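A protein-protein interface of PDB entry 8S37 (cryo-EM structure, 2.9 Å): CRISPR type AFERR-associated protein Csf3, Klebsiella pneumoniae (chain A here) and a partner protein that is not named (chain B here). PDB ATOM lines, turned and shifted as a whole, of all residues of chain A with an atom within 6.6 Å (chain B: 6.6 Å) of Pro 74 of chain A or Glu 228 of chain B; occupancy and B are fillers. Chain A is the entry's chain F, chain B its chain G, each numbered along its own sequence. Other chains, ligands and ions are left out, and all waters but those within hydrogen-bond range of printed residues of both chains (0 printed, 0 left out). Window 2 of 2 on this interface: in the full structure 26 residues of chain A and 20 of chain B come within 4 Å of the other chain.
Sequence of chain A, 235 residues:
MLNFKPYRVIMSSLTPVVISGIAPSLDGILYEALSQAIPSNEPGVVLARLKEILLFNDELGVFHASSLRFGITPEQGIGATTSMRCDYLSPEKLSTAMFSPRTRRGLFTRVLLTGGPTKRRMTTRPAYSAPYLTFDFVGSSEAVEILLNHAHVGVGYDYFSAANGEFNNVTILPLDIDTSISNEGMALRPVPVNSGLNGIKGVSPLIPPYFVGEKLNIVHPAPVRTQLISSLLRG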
ATOM      1  N   ILE A  72      28.615  -7.306   8.762  1.00  0.00           N
ATOM      2  CA  ILE A  72      29.132  -6.060   9.314  1.00  0.00           C
ATOM      3  C   ILE A  72      29.300  -6.227  10.817  1.00  0.00           C
ATOM      4  O   ILE A  72      28.376  -6.679  11.504  1.00  0.00           O
ATOM      5  CB  ILE A  72      28.223  -4.863   8.985  1.00  0.00           C
ATOM      6  CG1 ILE A  72      26.754  -5.179   9.283  1.00  0.00           C
ATOM      7  CG2 ILE A  72      28.402  -4.471   7.528  1.00  0.00           C
ATOM      8  CD1 ILE A  72      25.863  -3.972   9.281  1.00  0.00           C
ATOM      9  N   THR A  73      30.469  -5.881  11.315  1.00  0.00           N
ATOM     10  CA  THR A  73      30.747  -5.935  12.739  1.00  0.00           C
ATOM     11  C   THR A  73      30.493  -4.573  13.366  1.00  0.00           C
ATOM     12  O   THR A  73      30.443  -3.560  12.666  1.00  0.00           O
ATOM     13  CB  THR A  73      32.199  -6.342  12.972  1.00  0.00           C
ATOM     14  OG1 THR A  73      33.058  -5.241  12.649  1.00  0.00           O
ATOM     15  CG2 THR A  73      32.563  -7.528  12.103  1.00  0.00           C
ATOM     16  N   PRO A  74      30.317  -4.504  14.688  1.00  0.00           N
ATOM     17  CA  PRO A  74      30.131  -3.188  15.319  1.00  0.00           C
ATOM     18  C   PRO A  74      31.291  -2.234  15.098  1.00  0.00           C
ATOM     19  O   PRO A  74      31.108  -1.021  15.263  1.00  0.00           O
ATOM     20  CB  PRO A  74      29.954  -3.524  16.807  1.00  0.00           C
ATOM     21  CG  PRO A  74      30.418  -4.926  16.965  1.00  0.00           C
ATOM     22  CD  PRO A  74      30.164  -5.597  15.661  1.00  0.00           C
ATOM     23  N   GLU A  75      32.472  -2.731  14.730  1.00  0.00           N
ATOM     24  CA  GLU A  75      33.632  -1.872  14.523  1.00  0.00           C
ATOM     25  C   GLU A  75      33.753  -1.390  13.082  1.00  0.00           C
ATOM     26  O   GLU A  75      34.117  -0.232  12.854  1.00  0.00           O
ATOM     27  CB  GLU A  75      34.913  -2.610  14.922  1.00  0.00           C
ATOM     28  CG  GLU A  75      34.994  -2.982  16.398  1.00  0.00           C
ATOM     29  CD  GLU A  75      34.213  -4.237  16.737  1.00  0.00           C
ATOM     30  OE1 GLU A  75      33.458  -4.722  15.868  1.00  0.00           O
ATOM     31  OE2 GLU A  75      34.356  -4.741  17.871  1.00  0.00           O
ATOM     32  N   GLN A  76      33.457  -2.248  12.106  1.00  0.00           N
ATOM     33  CA  GLN A  76      33.500  -1.889  10.695  1.00  0.00           C
ATOM     34  C   GLN A  76      32.157  -2.200  10.053  1.00  0.00           C
ATOM     35  O   GLN A  76      31.561  -3.246  10.322  1.00  0.00           O
ATOM     36  CB  GLN A  76      34.614  -2.638   9.958  1.00  0.00           C
ATOM     37  CG  GLN A  76      34.853  -2.151   8.536  1.00  0.00           C
ATOM     38  CD  GLN A  76      35.902  -2.966   7.811  1.00  0.00           C
ATOM     39  OE1 GLN A  76      36.594  -3.783   8.416  1.00  0.00           O
ATOM     40  NE2 GLN A  76      36.024  -2.750   6.507  1.00  0.00           N
ATOM     41  N   GLY A  77      31.696  -1.293   9.187  1.00  0.00           N
ATOM     42  CA  GLY A  77      30.412  -1.418   8.539  1.00  0.00           C
ATOM     43  C   GLY A  77      30.532  -1.397   7.024  1.00  0.00           C
ATOM     44  O   GLY A  77      31.605  -1.166   6.457  1.00  0.00           O
ATOM     45  N   LEU A 228      24.505  -8.324  11.104  1.00  0.00           N
ATOM     46  CA  LEU A 228      25.521  -8.356  12.143  1.00  0.00           C
ATOM     47  C   LEU A 228      26.237  -9.699  12.121  1.00  0.00           C
ATOM     48  O   LEU A 228      25.610 -10.752  11.980  1.00  0.00           O
ATOM     49  CB  LEU A 228      24.893  -8.111  13.512  1.00  0.00           C
ATOM     50  CG  LEU A 228      24.608  -6.647  13.851  1.00  0.00           C
ATOM     51  CD1 LEU A 228      23.687  -6.553  15.056  1.00  0.00           C
ATOM     52  CD2 LEU A 228      25.902  -5.889  14.109  1.00  0.00           C
ATOM     53  N   ILE A 229      27.564  -9.658  12.252  1.00  0.00           N
ATOM     54  CA  ILE A 229      28.334 -10.896  12.250  1.00  0.00           C
ATOM     55  C   ILE A 229      27.916 -11.789  13.406  1.00  0.00           C
ATOM     56  O   ILE A 229      27.941 -13.020  13.292  1.00  0.00           O
ATOM     57  CB  ILE A 229      29.846 -10.598  12.284  1.00  0.00           C
ATOM     58  CG1 ILE A 229      30.632 -11.906  12.268  1.00  0.00           C
ATOM     59  CG2 ILE A 229      30.227  -9.788  13.522  1.00  0.00           C
ATOM     60  CD1 ILE A 229      31.996 -11.784  11.660  1.00  0.00           C
ATOM     61  N   SER A 230      27.532 -11.193  14.536  1.00  0.00           N
ATOM     62  CA  SER A 230      27.014 -11.988  15.643  1.00  0.00           C
ATOM     63  C   SER A 230      25.731 -12.702  15.244  1.00  0.00           C
ATOM     64  O   SER A 230      25.542 -13.882  15.558  1.00  0.00           O
ATOM     65  CB  SER A 230      26.776 -11.095  16.860  1.00  0.00           C
ATOM     66  OG  SER A 230      25.856 -10.062  16.555  1.00  0.00           O
ATOM     67  N   LEU B 220      29.267   6.911   8.074  1.00  0.00           N
ATOM     68  CA  LEU B 220      29.133   5.461   8.059  1.00  0.00           C
ATOM     69  C   LEU B 220      29.303   4.915   6.648  1.00  0.00           C
ATOM     70  O   LEU B 220      30.000   3.915   6.440  1.00  0.00           O
ATOM     71  CB  LEU B 220      27.779   5.059   8.635  1.00  0.00           C
ATOM     72  CG  LEU B 220      27.535   3.565   8.847  1.00  0.00           C
ATOM     73  CD1 LEU B 220      28.556   2.964   9.806  1.00  0.00           C
ATOM     74  CD2 LEU B 220      26.126   3.353   9.361  1.00  0.00           C
ATOM     75  N   ILE B 225      33.072   6.231  10.702  1.00  0.00           N
ATOM     76  CA  ILE B 225      32.633   5.969  12.067  1.00  0.00           C
ATOM     77  C   ILE B 225      32.177   4.522  12.152  1.00  0.00           C
ATOM     78  O   ILE B 225      31.581   3.992  11.208  1.00  0.00           O
ATOM     79  CB  ILE B 225      31.504   6.926  12.503  1.00  0.00           C
ATOM     80  CG1 ILE B 225      30.322   6.857  11.529  1.00  0.00           C
ATOM     81  CG2 ILE B 225      32.036   8.347  12.605  1.00  0.00           C
ATOM     82  CD1 ILE B 225      29.151   7.710  11.939  1.00  0.00           C
ATOM     83  N   THR B 226      32.460   3.887  13.282  1.00  0.00           N
ATOM     84  CA  THR B 226      32.091   2.496  13.458  1.00  0.00           C
ATOM     85  C   THR B 226      30.569   2.354  13.460  1.00  0.00           C
ATOM     86  O   THR B 226      29.855   3.286  13.838  1.00  0.00           O
ATOM     87  CB  THR B 226      32.655   1.949  14.765  1.00  0.00           C
ATOM     88  OG1 THR B 226      32.020   2.603  15.871  1.00  0.00           O
ATOM     89  CG2 THR B 226      34.158   2.175  14.840  1.00  0.00           C
ATOM     90  N   PRO B 227      30.042   1.202  13.030  1.00  0.00           N
ATOM     91  CA  PRO B 227      28.589   0.995  13.135  1.00  0.00           C
ATOM     92  C   PRO B 227      28.062   1.139  14.545  1.00  0.00           C
ATOM     93  O   PRO B 227      26.921   1.578  14.722  1.00  0.00           O
ATOM     94  CB  PRO B 227      28.406  -0.432  12.608  1.00  0.00           C
ATOM     95  CG  PRO B 227      29.491  -0.587  11.648  1.00  0.00           C
ATOM     96  CD  PRO B 227      30.669   0.118  12.254  1.00  0.00           C
ATOM     97  N   GLU B 228      28.847   0.774  15.557  1.00  0.00           N
ATOM     98  CA  GLU B 228      28.373   0.928  16.926  1.00  0.00           C
ATOM     99  C   GLU B 228      28.218   2.400  17.284  1.00  0.00           C
ATOM    100  O   GLU B 228      27.235   2.789  17.926  1.00  0.00           O
ATOM    101  CB  GLU B 228      29.341   0.225  17.882  1.00  0.00           C
ATOM    102  CG  GLU B 228      29.221   0.606  19.355  1.00  0.00           C
ATOM    103  CD  GLU B 228      27.820   0.437  19.901  1.00  0.00           C
ATOM    104  OE1 GLU B 228      27.020  -0.300  19.287  1.00  0.00           O
ATOM    105  OE2 GLU B 228      27.519   1.041  20.951  1.00  0.00           O
ATOM    106  N   ALA B 229      29.151   3.241  16.834  1.00  0.00           N
ATOM    107  CA  ALA B 229      29.019   4.671  17.079  1.00  0.00           C
ATOM    108  C   ALA B 229      27.807   5.240  16.356  1.00  0.00           C
ATOM    109  O   ALA B 229      27.059   6.046  16.924  1.00  0.00           O
ATOM    110  CB  ALA B 229      30.292   5.396  16.644  1.00  0.00           C
ATOM    111  N   ALA B 230      27.598   4.836  15.102  1.00  0.00           N
ATOM    112  CA  ALA B 230      26.444   5.323  14.355  1.00  0.00           C
ATOM    113  C   ALA B 230      25.139   4.881  15.004  1.00  0.00           C
ATOM    114  O   ALA B 230      24.183   5.658  15.078  1.00  0.00           O
ATOM    115  CB  ALA B 230      26.512   4.836  12.909  1.00  0.00           C
ATOM    116  N   SER B 231      25.076   3.634  15.469  1.00  0.00           N
ATOM    117  CA  SER B 231      23.865   3.153  16.121  1.00  0.00           C
ATOM    118  C   SER B 231      23.608   3.909  17.416  1.00  0.00           C
ATOM    119  O   SER B 231      22.461   4.260  17.718  1.00  0.00           O
ATOM    120  CB  SER B 231      23.972   1.653  16.385  1.00  0.00           C
ATOM    121  OG  SER B 231      24.991   1.374  17.326  1.00  0.00           O
ATOM    122  N   ASN B 232      24.662   4.171  18.190  1.00  0.00           N
ATOM    123  CA  ASN B 232      24.513   4.984  19.391  1.00  0.00           C
ATOM    124  C   ASN B 232      23.970   6.362  19.045  1.00  0.00           C
ATOM    125  O   ASN B 232      23.053   6.866  19.702  1.00  0.00           O
ATOM    126  CB  ASN B 232      25.850   5.097  20.119  1.00  0.00           C
ATOM    127  CG  ASN B 232      26.322   3.771  20.672  1.00  0.00           C
ATOM    128  OD1 ASN B 232      25.526   2.856  20.880  1.00  0.00           O
ATOM    129  ND2 ASN B 232      27.622   3.658  20.915  1.00  0.00           N
ATOM    130  N   GLU B 233      24.543   6.997  18.020  1.00  0.00           N
ATOM    131  CA  GLU B 233      24.104   8.336  17.643  1.00  0.00           C
ATOM    132  C   GLU B 233      22.647   8.335  17.187  1.00  0.00           C
ATOM    133  O   GLU B 233      21.873   9.224  17.560  1.00  0.00           O
ATOM    134  CB  GLU B 233      25.017   8.886  16.548  1.00  0.00           C
ATOM    135  CG  GLU B 233      24.909  10.389  16.332  1.00  0.00           C
ATOM    136  CD  GLU B 233      23.740  10.768  15.447  1.00  0.00           C
ATOM    137  OE1 GLU B 233      23.611  10.190  14.348  1.00  0.00           O
ATOM    138  OE2 GLU B 233      22.945  11.640  15.854  1.00  0.00           O
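O of Pro 74 of chain A sits at hydrogen-bond distance from N of Glu 228 of chain B (2.9 Å).
O of Pro 74 of chain A lies close to N of Pro 227 of chain B (3.3 Å).
Printed residues of chain B that touch a printed residue of chain A: Thr 226, Pro 227 and Glu 228.
The side-chain hydroxyl (OG1) of Thr 226 of chain B lies within hydrogen-bond range of the backbone NH (N) of Ala 229 of chain B (3.1 Å).
The side-chain hydroxyl (OG1) of Thr 73 of chain A is in hydrogen-bond range of the side-chain carboxylate (OE1) of Glu 75 of chain A (3.3 Å).
OG1 of Thr 73 of chain A sits at hydrogen-bond distance from N of Gln 76 of chain A (3.1 Å).
O of Glu 228 of chain B lies within hydrogen-bond range of OG of Ser 231 of chain B (2.7 Å).
The side-chain carboxylate (OE2) of Glu 228 of chain B sits at hydrogen-bond distance from the side-chain amide nitrogen (ND2) of Asn 232 of chain B (2.6 Å).
The backbone carbonyl oxygen (O) of Pro 227 of chain B sits at hydrogen-bond distance from the side-chain hydroxyl (OG) of Ser 231 of chain B, at 3.2 Å.
Of the printed residues of chain B, Thr 73 of chain A touches Pro 227.
Pro 74 of chain A touches just these residues of chain B: Thr 226, Pro 227 and Glu 228.
Printed residues of chain B within 4 Å of Glu 75 of chain A: Thr 226 and Pro 227.
Printed residues of chain A within 4 Å of Thr 226 of chain B: Pro 74 (3.4 Å) and Glu 75 (3.1 Å).
Of the printed residues of chain A, Pro 227 of chain B touches Thr 73 (3.3 Å), Pro 74 (3.2 Å), Glu 75 (3.5 Å), Gln 76 (3.5 Å) and Gly 77 (3.3 Å).
Glu 228 of chain B touches just one residue of chain A: Pro 74.
The nearest printed residue of chain B that does not touch Thr 73 of chain A is Glu 228 of chain B (5.4 Å).
Among the printed residues, pairs that only touch across the chains: Glu 75 of chain A with Thr 226 of chain B (3.1 Å), Thr 73 of chain A with Pro 227 of chain B (3.3 Å), Gly 77 of chain A with Pro 227 of chain B (3.3 Å), Pro 74 of chain A with Thr 226 of chain B (3.4 Å), Gln 76 of chain A with Pro 227 of chain B (3.5 Å) and Glu 75 of chain A with Pro 227 of chain B (3.5 Å).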
